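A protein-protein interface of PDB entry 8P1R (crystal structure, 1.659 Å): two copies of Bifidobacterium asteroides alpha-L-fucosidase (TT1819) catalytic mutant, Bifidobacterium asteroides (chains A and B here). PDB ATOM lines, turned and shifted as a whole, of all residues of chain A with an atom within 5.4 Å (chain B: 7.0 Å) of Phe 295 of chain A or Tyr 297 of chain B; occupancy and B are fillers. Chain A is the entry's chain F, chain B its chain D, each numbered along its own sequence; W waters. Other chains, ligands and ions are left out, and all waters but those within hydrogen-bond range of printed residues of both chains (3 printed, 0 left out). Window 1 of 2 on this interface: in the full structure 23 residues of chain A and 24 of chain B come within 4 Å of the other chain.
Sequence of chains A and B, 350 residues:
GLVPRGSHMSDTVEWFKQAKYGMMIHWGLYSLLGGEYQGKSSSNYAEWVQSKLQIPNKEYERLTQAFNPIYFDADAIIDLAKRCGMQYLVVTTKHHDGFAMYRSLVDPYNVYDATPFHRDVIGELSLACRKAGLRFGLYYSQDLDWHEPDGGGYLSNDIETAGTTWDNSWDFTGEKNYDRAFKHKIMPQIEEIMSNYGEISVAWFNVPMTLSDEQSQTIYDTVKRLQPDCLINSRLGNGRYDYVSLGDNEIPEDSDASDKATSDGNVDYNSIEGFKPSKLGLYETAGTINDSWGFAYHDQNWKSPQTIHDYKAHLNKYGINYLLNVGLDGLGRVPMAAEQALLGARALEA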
ATOM      1  N   HIS A  26     -23.736  35.535 -10.072  1.00  0.00           N
ATOM      2  CA  HIS A  26     -22.523  36.358  -9.991  1.00  0.00           C
ATOM      3  C   HIS A  26     -22.043  36.618 -11.420  1.00  0.00           C
ATOM      4  O   HIS A  26     -21.818  35.654 -12.146  1.00  0.00           O
ATOM      5  CB  HIS A  26     -21.377  35.693  -9.205  1.00  0.00           C
ATOM      6  CG  HIS A  26     -21.557  35.738  -7.741  1.00  0.00           C
ATOM      7  ND1 HIS A  26     -22.595  35.077  -7.109  1.00  0.00           N
ATOM      8  CD2 HIS A  26     -20.835  36.413  -6.811  1.00  0.00           C
ATOM      9  CE1 HIS A  26     -22.425  35.319  -5.792  1.00  0.00           C
ATOM     10  NE2 HIS A  26     -21.395  36.153  -5.587  1.00  0.00           N
ATOM     11  N   TYR A  30     -14.697  40.244 -13.460  1.00  0.00           N
ATOM     12  CA  TYR A  30     -13.963  39.075 -13.008  1.00  0.00           C
ATOM     13  C   TYR A  30     -14.309  37.843 -13.845  1.00  0.00           C
ATOM     14  O   TYR A  30     -13.505  36.914 -13.965  1.00  0.00           O
ATOM     15  CB  TYR A  30     -14.191  38.843 -11.514  1.00  0.00           C
ATOM     16  CG  TYR A  30     -15.635  38.906 -11.076  1.00  0.00           C
ATOM     17  CD1 TYR A  30     -16.496  37.821 -11.247  1.00  0.00           C
ATOM     18  CD2 TYR A  30     -16.131  40.027 -10.434  1.00  0.00           C
ATOM     19  CE1 TYR A  30     -17.822  37.868 -10.838  1.00  0.00           C
ATOM     20  CE2 TYR A  30     -17.463  40.129 -10.085  1.00  0.00           C
ATOM     21  CZ  TYR A  30     -18.307  39.031 -10.245  1.00  0.00           C
ATOM     22  OH  TYR A  30     -19.637  39.053  -9.843  1.00  0.00           O
ATOM     23  N   SER A  31     -15.527  37.798 -14.397  1.00  0.00           N
ATOM     24  CA  SER A  31     -15.967  36.658 -15.175  1.00  0.00           C
ATOM     25  C   SER A  31     -15.151  36.499 -16.466  1.00  0.00           C
ATOM     26  O   SER A  31     -14.994  35.372 -16.953  1.00  0.00           O
ATOM     27  CB  SER A  31     -17.415  36.809 -15.496  1.00  0.00           C
ATOM     28  OG  SER A  31     -18.206  37.096 -14.341  1.00  0.00           O
ATOM     29  N   GLY A  34     -11.972  34.728 -15.389  1.00  0.00           N
ATOM     30  CA  GLY A  34     -12.318  33.331 -15.189  1.00  0.00           C
ATOM     31  C   GLY A  34     -11.325  32.609 -14.302  1.00  0.00           C
ATOM     32  O   GLY A  34     -11.085  31.419 -14.507  1.00  0.00           O
ATOM     33  N   GLY A  35     -10.767  33.315 -13.317  1.00  0.00           N
ATOM     34  CA  GLY A  35      -9.928  32.661 -12.312  1.00  0.00           C
ATOM     35  C   GLY A  35      -8.440  32.634 -12.654  1.00  0.00           C
ATOM     36  O   GLY A  35      -7.696  32.003 -11.932  1.00  0.00           O
ATOM     37  N   ALA A  46     -13.074  32.845  -7.900  1.00  0.00           N
ATOM     38  CA  ALA A  46     -12.554  33.584  -9.034  1.00  0.00           C
ATOM     39  C   ALA A  46     -12.960  35.060  -8.954  1.00  0.00           C
ATOM     40  O   ALA A  46     -12.285  35.944  -9.504  1.00  0.00           O
ATOM     41  CB  ALA A  46     -13.048  32.925 -10.307  1.00  0.00           C
ATOM     42  N   SER A 292     -16.778  27.801  -7.116  1.00  0.00           N
ATOM     43  CA  SER A 292     -16.570  29.229  -7.277  1.00  0.00           C
ATOM     44  C   SER A 292     -17.923  29.919  -7.377  1.00  0.00           C
ATOM     45  O   SER A 292     -18.885  29.312  -7.860  1.00  0.00           O
ATOM     46  CB  SER A 292     -15.713  29.558  -8.495  1.00  0.00           C
ATOM     47  OG  SER A 292     -15.347  30.987  -8.564  1.00  0.00           O
ATOM     48  N   TRP A 293     -17.962  31.198  -6.994  1.00  0.00           N
ATOM     49  CA  TRP A 293     -19.139  32.030  -7.218  1.00  0.00           C
ATOM     50  C   TRP A 293     -19.090  32.615  -8.622  1.00  0.00           C
ATOM     51  O   TRP A 293     -19.995  32.411  -9.417  1.00  0.00           O
ATOM     52  CB  TRP A 293     -19.319  33.091  -6.106  1.00  0.00           C
ATOM     53  CG  TRP A 293     -19.524  32.436  -4.777  1.00  0.00           C
ATOM     54  CD1 TRP A 293     -18.523  32.128  -3.917  1.00  0.00           C
ATOM     55  CD2 TRP A 293     -20.751  31.966  -4.165  1.00  0.00           C
ATOM     56  NE1 TRP A 293     -19.025  31.405  -2.852  1.00  0.00           N
ATOM     57  CE2 TRP A 293     -20.400  31.356  -2.953  1.00  0.00           C
ATOM     58  CE3 TRP A 293     -22.107  32.055  -4.499  1.00  0.00           C
ATOM     59  CZ2 TRP A 293     -21.349  30.803  -2.086  1.00  0.00           C
ATOM     60  CZ3 TRP A 293     -23.046  31.504  -3.642  1.00  0.00           C
ATOM     61  CH2 TRP A 293     -22.681  30.896  -2.446  1.00  0.00           C
ATOM     62  N   GLY A 294     -18.019  33.352  -8.916  1.00  0.00           N
ATOM     63  CA  GLY A 294     -17.728  33.806 -10.273  1.00  0.00           C
ATOM     64  C   GLY A 294     -17.339  32.618 -11.141  1.00  0.00           C
ATOM     65  O   GLY A 294     -16.847  31.606 -10.667  1.00  0.00           O
ATOM     66  N   PHE A 295     -17.531  32.774 -12.438  1.00  0.00           N
ATOM     67  CA  PHE A 295     -17.063  31.809 -13.425  1.00  0.00           C
ATOM     68  C   PHE A 295     -15.555  31.581 -13.275  1.00  0.00           C
ATOM     69  O   PHE A 295     -14.776  32.503 -13.110  1.00  0.00           O
ATOM     70  CB  PHE A 295     -17.375  32.365 -14.808  1.00  0.00           C
ATOM     71  CG  PHE A 295     -16.907  31.449 -15.905  1.00  0.00           C
ATOM     72  CD1 PHE A 295     -17.558  30.242 -16.124  1.00  0.00           C
ATOM     73  CD2 PHE A 295     -15.786  31.765 -16.662  1.00  0.00           C
ATOM     74  CE1 PHE A 295     -17.146  29.386 -17.142  1.00  0.00           C
ATOM     75  CE2 PHE A 295     -15.377  30.914 -17.670  1.00  0.00           C
ATOM     76  CZ  PHE A 295     -16.018  29.712 -17.883  1.00  0.00           C
ATOM     77  N   ALA A 296     -15.162  30.320 -13.319  1.00  0.00           N
ATOM     78  CA  ALA A 296     -13.792  29.895 -13.180  1.00  0.00           C
ATOM     79  C   ALA A 296     -13.503  28.797 -14.204  1.00  0.00           C
ATOM     80  O   ALA A 296     -13.974  27.690 -14.002  1.00  0.00           O
ATOM     81  CB  ALA A 296     -13.569  29.416 -11.765  1.00  0.00           C
ATOM     82  N   TYR A 297     -12.682  29.125 -15.208  1.00  0.00           N
ATOM     83  CA  TYR A 297     -12.431  28.247 -16.343  1.00  0.00           C
ATOM     84  C   TYR A 297     -11.933  26.883 -15.815  1.00  0.00           C
ATOM     85  O   TYR A 297     -12.358  25.822 -16.288  1.00  0.00           O
ATOM     86  CB  TYR A 297     -11.647  29.086 -17.387  1.00  0.00           C
ATOM     87  CG  TYR A 297     -10.450  28.403 -17.958  1.00  0.00           C
ATOM     88  CD1 TYR A 297     -10.519  27.051 -18.175  1.00  0.00           C
ATOM     89  CD2 TYR A 297      -9.253  29.057 -18.271  1.00  0.00           C
ATOM     90  CE1 TYR A 297      -9.435  26.346 -18.644  1.00  0.00           C
ATOM     91  CE2 TYR A 297      -8.160  28.371 -18.766  1.00  0.00           C
ATOM     92  CZ  TYR A 297      -8.260  26.992 -18.919  1.00  0.00           C
ATOM     93  OH  TYR A 297      -7.369  26.040 -19.321  1.00  0.00           O
ATOM     94  N   GLN A 300     -14.003  22.477 -12.795  1.00  0.00           N
ATOM     95  CA  GLN A 300     -14.983  21.589 -13.402  1.00  0.00           C
ATOM     96  C   GLN A 300     -15.555  20.657 -12.339  1.00  0.00           C
ATOM     97  O   GLN A 300     -16.082  19.581 -12.635  1.00  0.00           O
ATOM     98  CB  GLN A 300     -14.365  20.809 -14.572  1.00  0.00           C
ATOM     99  CG  GLN A 300     -13.867  21.709 -15.721  1.00  0.00           C
ATOM    100  CD  GLN A 300     -14.932  22.576 -16.352  1.00  0.00           C
ATOM    101  OE1 GLN A 300     -16.092  22.189 -16.528  1.00  0.00           O
ATOM    102  NE2 GLN A 300     -14.584  23.830 -16.626  1.00  0.00           N
ATOM    103  N   GLY A 327     -22.486  31.212 -12.047  1.00  0.00           N
ATOM    104  CA  GLY A 327     -21.525  32.246 -12.409  1.00  0.00           C
ATOM    105  C   GLY A 327     -21.441  32.344 -13.929  1.00  0.00           C
ATOM    106  O   GLY A 327     -20.902  31.439 -14.562  1.00  0.00           O
ATOM    107  N   LEU A 328     -22.032  33.390 -14.511  1.00  0.00           N
ATOM    108  CA  LEU A 328     -22.076  33.501 -15.960  1.00  0.00           C
ATOM    109  C   LEU A 328     -20.663  33.703 -16.503  1.00  0.00           C
ATOM    110  O   LEU A 328     -19.825  34.330 -15.853  1.00  0.00           O
ATOM    111  CB  LEU A 328     -22.960  34.680 -16.391  1.00  0.00           C
ATOM    112  CG  LEU A 328     -24.420  34.631 -15.948  1.00  0.00           C
ATOM    113  CD1 LEU A 328     -25.131  35.879 -16.346  1.00  0.00           C
ATOM    114  CD2 LEU A 328     -25.147  33.446 -16.539  1.00  0.00           C
ATOM    115  N   ASP A 329     -20.429  33.200 -17.722  1.00  0.00           N
ATOM    116  CA  ASP A 329     -19.117  33.326 -18.346  1.00  0.00           C
ATOM    117  C   ASP A 329     -18.985  34.709 -18.982  1.00  0.00           C
ATOM    118  O   ASP A 329     -19.865  35.566 -18.902  1.00  0.00           O
ATOM    119  CB  ASP A 329     -18.839  32.164 -19.309  1.00  0.00           C
ATOM    120  CG  ASP A 329     -19.593  32.182 -20.615  1.00  0.00           C
ATOM    121  OD1 ASP A 329     -20.244  33.203 -20.903  1.00  0.00           O
ATOM    122  OD2 ASP A 329     -19.521  31.132 -21.317  1.00  0.00           O
ATOM    123  N   GLY A 330     -17.816  34.949 -19.613  1.00  0.00           N
ATOM    124  CA  GLY A 330     -17.534  36.246 -20.203  1.00  0.00           C
ATOM    125  C   GLY A 330     -18.439  36.608 -21.367  1.00  0.00           C
ATOM    126  O   GLY A 330     -18.482  37.779 -21.782  1.00  0.00           O
ATOM    127  N   ARG A 333     -23.115  33.617 -20.680  1.00  0.00           N
ATOM    128  CA  ARG A 333     -23.799  32.329 -20.771  1.00  0.00           C
ATOM    129  C   ARG A 333     -23.782  31.630 -19.400  1.00  0.00           C
ATOM    130  O   ARG A 333     -22.817  31.699 -18.635  1.00  0.00           O
ATOM    131  CB  ARG A 333     -23.082  31.406 -21.753  1.00  0.00           C
ATOM    132  CG  ARG A 333     -22.850  32.030 -23.120  1.00  0.00           C
ATOM    133  CD  ARG A 333     -22.243  31.051 -24.098  1.00  0.00           C
ATOM    134  NE  ARG A 333     -20.814  30.828 -23.768  1.00  0.00           N
ATOM    135  CZ  ARG A 333     -20.050  30.003 -24.462  1.00  0.00           C
ATOM    136  NH1 ARG A 333     -20.485  29.517 -25.617  1.00  0.00           N
ATOM    137  NH2 ARG A 333     -18.868  29.627 -23.999  1.00  0.00           N
ATOM    138  N   PRO A 335     -22.833  28.357 -17.897  1.00  0.00           N
ATOM    139  CA  PRO A 335     -21.966  27.293 -18.378  1.00  0.00           C
ATOM    140  C   PRO A 335     -22.810  26.059 -18.624  1.00  0.00           C
ATOM    141  O   PRO A 335     -23.744  25.768 -17.870  1.00  0.00           O
ATOM    142  CB  PRO A 335     -20.992  27.068 -17.232  1.00  0.00           C
ATOM    143  CG  PRO A 335     -20.877  28.473 -16.675  1.00  0.00           C
ATOM    144  CD  PRO A 335     -22.305  28.992 -16.676  1.00  0.00           C
ATOM    145  N   SER B  31     -12.360  30.061 -30.404  1.00  0.00           N
ATOM    146  CA  SER B  31     -11.735  30.192 -29.086  1.00  0.00           C
ATOM    147  C   SER B  31     -12.656  30.892 -28.090  1.00  0.00           C
ATOM    148  O   SER B  31     -12.592  30.614 -26.884  1.00  0.00           O
ATOM    149  CB  SER B  31     -10.440  30.939 -29.211  1.00  0.00           C
ATOM    150  OG  SER B  31      -9.608  30.370 -30.236  1.00  0.00           O
ATOM    151  N   LEU B  32     -13.492  31.826 -28.579  1.00  0.00           N
ATOM    152  CA  LEU B  32     -14.472  32.487 -27.737  1.00  0.00           C
ATOM    153  C   LEU B  32     -15.510  31.496 -27.197  1.00  0.00           C
ATOM    154  O   LEU B  32     -15.835  31.545 -26.009  1.00  0.00           O
ATOM    155  CB  LEU B  32     -15.154  33.575 -28.554  1.00  0.00           C
ATOM    156  CG  LEU B  32     -14.324  34.806 -28.889  1.00  0.00           C
ATOM    157  CD1 LEU B  32     -15.041  35.650 -29.906  1.00  0.00           C
ATOM    158  CD2 LEU B  32     -14.042  35.635 -27.620  1.00  0.00           C
ATOM    159  N   LEU B  33     -15.979  30.580 -28.058  1.00  0.00           N
ATOM    160  CA  LEU B  33     -16.985  29.617 -27.652  1.00  0.00           C
ATOM    161  C   LEU B  33     -16.387  28.609 -26.668  1.00  0.00           C
ATOM    162  O   LEU B  33     -17.078  28.124 -25.780  1.00  0.00           O
ATOM    163  CB  LEU B  33     -17.544  28.901 -28.879  1.00  0.00           C
ATOM    164  CG  LEU B  33     -18.429  29.745 -29.778  1.00  0.00           C
ATOM    165  CD1 LEU B  33     -18.910  28.964 -31.009  1.00  0.00           C
ATOM    166  CD2 LEU B  33     -19.634  30.279 -29.028  1.00  0.00           C
ATOM    167  N   GLY B  34     -15.115  28.244 -26.878  1.00  0.00           N
ATOM    168  CA  GLY B  34     -14.427  27.409 -25.913  1.00  0.00           C
ATOM    169  C   GLY B  34     -15.075  26.040 -25.742  1.00  0.00           C
ATOM    170  O   GLY B  34     -14.989  25.467 -24.673  1.00  0.00           O
ATOM    171  N   GLY B  35     -15.658  25.491 -26.815  1.00  0.00           N
ATOM    172  CA  GLY B  35     -16.168  24.124 -26.774  1.00  0.00           C
ATOM    173  C   GLY B  35     -17.635  24.031 -26.380  1.00  0.00           C
ATOM    174  O   GLY B  35     -18.085  22.915 -26.093  1.00  0.00           O
ATOM    175  N   GLU B  36     -18.331  25.159 -26.260  1.00  0.00           N
ATOM    176  CA  GLU B  36     -19.755  25.161 -25.945  1.00  0.00           C
ATOM    177  C   GLU B  36     -20.465  26.160 -26.834  1.00  0.00           C
ATOM    178  O   GLU B  36     -19.925  27.233 -27.140  1.00  0.00           O
ATOM    179  CB  GLU B  36     -20.052  25.628 -24.496  1.00  0.00           C
ATOM    180  CG  GLU B  36     -19.388  24.778 -23.493  1.00  0.00           C
ATOM    181  CD  GLU B  36     -19.614  25.159 -22.037  1.00  0.00           C
ATOM    182  OE1 GLU B  36     -20.474  26.062 -21.745  1.00  0.00           O
ATOM    183  OE2 GLU B  36     -18.868  24.606 -21.243  1.00  0.00           O
ATOM    184  N   ALA B  46     -12.608  21.496 -29.953  1.00  0.00           N
ATOM    185  CA  ALA B  46     -13.450  22.682 -29.808  1.00  0.00           C
ATOM    186  C   ALA B  46     -13.442  23.545 -31.070  1.00  0.00           C
ATOM    187  O   ALA B  46     -14.409  24.262 -31.344  1.00  0.00           O
ATOM    188  CB  ALA B  46     -12.993  23.467 -28.591  1.00  0.00           C
ATOM    189  N   ASN B 290      -3.789  19.514 -23.809  1.00  0.00           N
ATOM    190  CA  ASN B 290      -5.010  18.787 -23.466  1.00  0.00           C
ATOM    191  C   ASN B 290      -5.456  18.022 -24.721  1.00  0.00           C
ATOM    192  O   ASN B 290      -4.597  17.558 -25.452  1.00  0.00           O
ATOM    193  CB  ASN B 290      -6.069  19.702 -22.819  1.00  0.00           C
ATOM    194  CG  ASN B 290      -6.563  20.846 -23.676  1.00  0.00           C
ATOM    195  OD1 ASN B 290      -6.156  21.036 -24.842  1.00  0.00           O
ATOM    196  ND2 ASN B 290      -7.453  21.638 -23.081  1.00  0.00           N
ATOM    197  N   GLY B 294      -8.220  23.953 -30.503  1.00  0.00           N
ATOM    198  CA  GLY B 294      -8.750  25.187 -29.970  1.00  0.00           C
ATOM    199  C   GLY B 294      -8.958  25.115 -28.468  1.00  0.00           C
ATOM    200  O   GLY B 294      -9.099  24.030 -27.882  1.00  0.00           O
ATOM    201  N   PHE B 295      -8.960  26.295 -27.841  1.00  0.00           N
ATOM    202  CA  PHE B 295      -9.273  26.429 -26.428  1.00  0.00           C
ATOM    203  C   PHE B 295     -10.619  25.793 -26.097  1.00  0.00           C
ATOM    204  O   PHE B 295     -11.594  25.954 -26.839  1.00  0.00           O
ATOM    205  CB  PHE B 295      -9.302  27.908 -26.076  1.00  0.00           C
ATOM    206  CG  PHE B 295      -9.654  28.182 -24.644  1.00  0.00           C
ATOM    207  CD1 PHE B 295      -8.762  27.837 -23.620  1.00  0.00           C
ATOM    208  CD2 PHE B 295     -10.915  28.663 -24.300  1.00  0.00           C
ATOM    209  CE1 PHE B 295      -9.083  28.049 -22.290  1.00  0.00           C
ATOM    210  CE2 PHE B 295     -11.213  28.898 -22.970  1.00  0.00           C
ATOM    211  CZ  PHE B 295     -10.296  28.606 -21.965  1.00  0.00           C
ATOM    212  N   ALA B 296     -10.640  25.040 -25.013  1.00  0.00           N
ATOM    213  CA  ALA B 296     -11.830  24.301 -24.608  1.00  0.00           C
ATOM    214  C   ALA B 296     -11.972  24.420 -23.076  1.00  0.00           C
ATOM    215  O   ALA B 296     -11.262  23.740 -22.385  1.00  0.00           O
ATOM    216  CB  ALA B 296     -11.700  22.869 -25.031  1.00  0.00           C
ATOM    217  N   TYR B 297     -12.957  25.232 -22.650  1.00  0.00           N
ATOM    218  CA  TYR B 297     -13.204  25.568 -21.251  1.00  0.00           C
ATOM    219  C   TYR B 297     -13.212  24.300 -20.388  1.00  0.00           C
ATOM    220  O   TYR B 297     -12.603  24.193 -19.332  1.00  0.00           O
ATOM    221  CB  TYR B 297     -14.545  26.322 -21.139  1.00  0.00           C
ATOM    222  CG  TYR B 297     -14.598  27.794 -21.496  1.00  0.00           C
ATOM    223  CD1 TYR B 297     -13.947  28.718 -20.713  1.00  0.00           C
ATOM    224  CD2 TYR B 297     -15.401  28.296 -22.524  1.00  0.00           C
ATOM    225  CE1 TYR B 297     -13.995  30.071 -20.996  1.00  0.00           C
ATOM    226  CE2 TYR B 297     -15.457  29.650 -22.835  1.00  0.00           C
ATOM    227  CZ  TYR B 297     -14.747  30.546 -22.052  1.00  0.00           C
ATOM    228  OH  TYR B 297     -14.680  31.908 -22.214  1.00  0.00           O
ATOM    229  N   HIS B 298     -13.939  23.285 -20.826  1.00  0.00           N
ATOM    230  CA  HIS B 298     -14.234  22.122 -20.005  1.00  0.00           C
ATOM    231  C   HIS B 298     -13.255  20.971 -20.190  1.00  0.00           C
ATOM    232  O   HIS B 298     -13.434  19.982 -19.515  1.00  0.00           O
ATOM    233  CB  HIS B 298     -15.700  21.729 -20.019  1.00  0.00           C
ATOM    234  CG  HIS B 298     -16.289  21.425 -21.302  1.00  0.00           C
ATOM    235  ND1 HIS B 298     -15.919  20.390 -22.132  1.00  0.00           N
ATOM    236  CD2 HIS B 298     -17.370  22.046 -21.880  1.00  0.00           C
ATOM    237  CE1 HIS B 298     -16.720  20.402 -23.218  1.00  0.00           C
ATOM    238  NE2 HIS B 298     -17.627  21.390 -23.078  1.00  0.00           N
ATOM    239  N   ASP B 299     -12.172  21.141 -20.961  1.00  0.00           N
ATOM    240  CA  ASP B 299     -11.132  20.127 -21.069  1.00  0.00           C
ATOM    241  C   ASP B 299      -9.954  20.496 -20.170  1.00  0.00           C
ATOM    242  O   ASP B 299      -9.153  21.353 -20.529  1.00  0.00           O
ATOM    243  CB  ASP B 299     -10.684  19.999 -22.513  1.00  0.00           C
ATOM    244  CG  ASP B 299      -9.556  18.990 -22.763  1.00  0.00           C
ATOM    245  OD1 ASP B 299      -9.077  18.404 -21.788  1.00  0.00           O
ATOM    246  OD2 ASP B 299      -9.182  18.817 -23.979  1.00  0.00           O
ATOM    247  N   GLN B 300      -9.872  19.849 -19.006  1.00  0.00           N
ATOM    248  CA  GLN B 300      -8.763  20.068 -18.074  1.00  0.00           C
ATOM    249  C   GLN B 300      -7.840  18.848 -18.055  1.00  0.00           C
ATOM    250  O   GLN B 300      -7.095  18.647 -17.102  1.00  0.00           O
ATOM    251  CB  GLN B 300      -9.280  20.366 -16.653  1.00  0.00           C
ATOM    252  CG  GLN B 300     -10.108  21.653 -16.586  1.00  0.00           C
ATOM    253  CD  GLN B 300      -9.389  22.915 -17.051  1.00  0.00           C
ATOM    254  OE1 GLN B 300      -8.210  23.157 -16.779  1.00  0.00           O
ATOM    255  NE2 GLN B 300     -10.086  23.746 -17.784  1.00  0.00           N
ATOM    256  N   TRP B 302      -4.947  18.080 -19.020  1.00  0.00           N
ATOM    257  CA  TRP B 302      -3.631  18.562 -19.409  1.00  0.00           C
ATOM    258  C   TRP B 302      -2.621  17.446 -19.181  1.00  0.00           C
ATOM    259  O   TRP B 302      -2.547  16.859 -18.091  1.00  0.00           O
ATOM    260  CB  TRP B 302      -3.223  19.808 -18.616  1.00  0.00           C
ATOM    261  CG  TRP B 302      -4.187  20.946 -18.720  1.00  0.00           C
ATOM    262  CD1 TRP B 302      -5.168  21.283 -17.810  1.00  0.00           C
ATOM    263  CD2 TRP B 302      -4.360  21.830 -19.843  1.00  0.00           C
ATOM    264  NE1 TRP B 302      -5.925  22.302 -18.312  1.00  0.00           N
ATOM    265  CE2 TRP B 302      -5.425  22.694 -19.532  1.00  0.00           C
ATOM    266  CE3 TRP B 302      -3.712  21.999 -21.062  1.00  0.00           C
ATOM    267  CZ2 TRP B 302      -5.810  23.712 -20.383  1.00  0.00           C
ATOM    268  CZ3 TRP B 302      -4.119  22.983 -21.929  1.00  0.00           C
ATOM    269  CH2 TRP B 302      -5.155  23.836 -21.589  1.00  0.00           C
ATOM    270  N   ASP B 329      -6.939  31.413 -25.381  1.00  0.00           N
ATOM    271  CA  ASP B 329      -8.311  31.690 -24.976  1.00  0.00           C
ATOM    272  C   ASP B 329      -8.834  32.934 -25.701  1.00  0.00           C
ATOM    273  O   ASP B 329      -8.167  33.560 -26.530  1.00  0.00           O
ATOM    274  CB  ASP B 329      -8.399  31.754 -23.455  1.00  0.00           C
ATOM    275  CG  ASP B 329      -7.880  33.003 -22.788  1.00  0.00           C
ATOM    276  OD1 ASP B 329      -7.523  33.943 -23.515  1.00  0.00           O
ATOM    277  OD2 ASP B 329      -7.859  33.023 -21.567  1.00  0.00           O
ATOM    278  N   GLY B 330     -10.081  33.288 -25.393  1.00  0.00           N
ATOM    279  CA  GLY B 330     -10.743  34.394 -26.056  1.00  0.00           C
ATOM    280  C   GLY B 330     -10.139  35.748 -25.753  1.00  0.00           C
ATOM    281  O   GLY B 330     -10.423  36.723 -26.477  1.00  0.00           O
HETATM  282  O   HOH W   1     -19.596  28.508 -20.426  1.00  0.00           O
HETATM  283  O   HOH W   2     -15.201  33.938 -19.719  1.00  0.00           O
HETATM  284  O   HOH W   3      -9.118  24.266 -20.842  1.00  0.00           O
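Of the printed residues of chain B, Phe 295 of chain A touches Tyr 297 (3.6 Å).
Of the printed residues of chain B, Tyr 297 of chain A touches Phe 295 (3.6 Å), Tyr 297 (3.5 Å), Gln 300 (2.8 Å) and Trp 302 (3.0 Å).
Of the printed residues of chain B, Pro 335 of chain A touches Glu 36.
Printed residues of chain A within 4 Å of Tyr 297 of chain B: Phe 295 (3.6 Å), Tyr 297 (3.5 Å), Gln 300 (3.4 Å) and Arg 333 (3.6 Å).
The nearest printed residue of chain B that does not touch Phe 295 of chain A is Glu 36 of chain B (6.5 Å).
Water W3 lies within hydrogen-bond range of O of Ala 296 of chain B (2.7 Å), OH of Tyr 297 of chain A (2.9 Å), O of Asp 299 of chain B (2.9 Å) and NE2 of Gln 300 of chain B (3.2 Å).
Water W1 bridges OD2 of Asp 329 of chain A (2.8 Å) and OE1 of Glu 36 of chain B (2.9 Å).
Water W2 lies within hydrogen-bond range of N of Gly 330 of chain A (2.8 Å), O of Ser 31 of chain A (3.1 Å) and OH of Tyr 297 of chain B (3.3 Å).
The backbone carbonyl oxygen of Leu 33 of chain B sits at hydrogen-bond distance from the guanidinium group of Arg 333 of chain A, at 2.9 Å.
The guanidinium group of Arg 333 of chain A sits at hydrogen-bond distance from the backbone carbonyl oxygen of Glu 36 of chain B (2.8 Å).
O of Tyr 297 of chain B lies within hydrogen-bond range of NE2 of Gln 300 of chain A, at 3.4 Å.
The side-chain amide nitrogen (NE2) of Gln 300 of chain B lies close to the backbone carbonyl oxygen (O) of Tyr 297 of chain A (3.4 Å).
The backbone carbonyl oxygen (O) of Tyr 297 of chain A sits close to the backbone carbonyl oxygen (O) of Tyr 297 of chain B, at 3.5 Å.
Phe 295 of chain A touches Tyr 297 of chain B, and with the chains exchanged Tyr 297 of chain A touches Phe 295 of chain B.
Tyr 297 of chain A touches its own counterpart, Tyr 297 of chain B.
Tyr 297 of chain A touches Gln 300 of chain B, and with the chains exchanged Gln 300 of chain A touches Tyr 297 of chain B.
Gln 300 of chain A touches its own counterpart, Gln 300 of chain B.
11 positions are printed for both chains.
Of the 19 printed residues of chain A, 5 touch a printed residue of chain B.
Printed residues of chain A that touch a printed residue of chain B: Phe 295, Tyr 297, Gln 300, Arg 333 and Pro 335.
Of the 18 printed residues of chain B, 7 touch a printed residue of chain A.
Hydrophobic or aromatic side chains of chain B that line the printed part of chain A: Leu 33, Phe 295, Tyr 297, His 298 and Trp 302.
Among the printed residues, no Asp or Glu carboxylate lies within 4 Å of a Lys or Arg side-chain nitrogen of the other chain.
The backbone carbonyl oxygen (O) of Gly 34 of chain B lies within hydrogen-bond range of the backbone NH (N) of Tyr 297 of chain B (2.9 Å).
A ring nitrogen (NE2) of His 298 of chain B is in hydrogen-bond range of the backbone carbonyl oxygen of Gly 35 of chain B (3.4 Å).
OE1 of Gln 300 of chain B is in hydrogen-bond range of NE1 of Trp 302 of chain B, at 2.9 Å.
The backbone NH (N) of Tyr 297 of chain A lies within hydrogen-bond range of the backbone carbonyl oxygen (O) of Gly 34 of chain A (2.9 Å).
The backbone carbonyl oxygen of Tyr 297 of chain A is in hydrogen-bond range of the side-chain amide nitrogen of Gln 300 of chain A, at 3.0 Å.
The guanidinium group of Arg 333 of chain A is in salt-bridge range of the side-chain carboxylate of Asp 329 of chain A, at 2.8 Å.
Among the printed residues, merely in contact across the chains: Tyr 297 of chain A with Trp 302 of chain B, Gln 300 of chain A with His 298 of chain B, Arg 333 of chain A with Tyr 297 of chain B, Tyr 297 of chain A with Phe 295 of chain B, Phe 295 of chain A with Tyr 297 of chain B, Gln 300 of chain A with Gln 300 of chain B and Pro 335 of chain A with Glu 36 of chain B.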
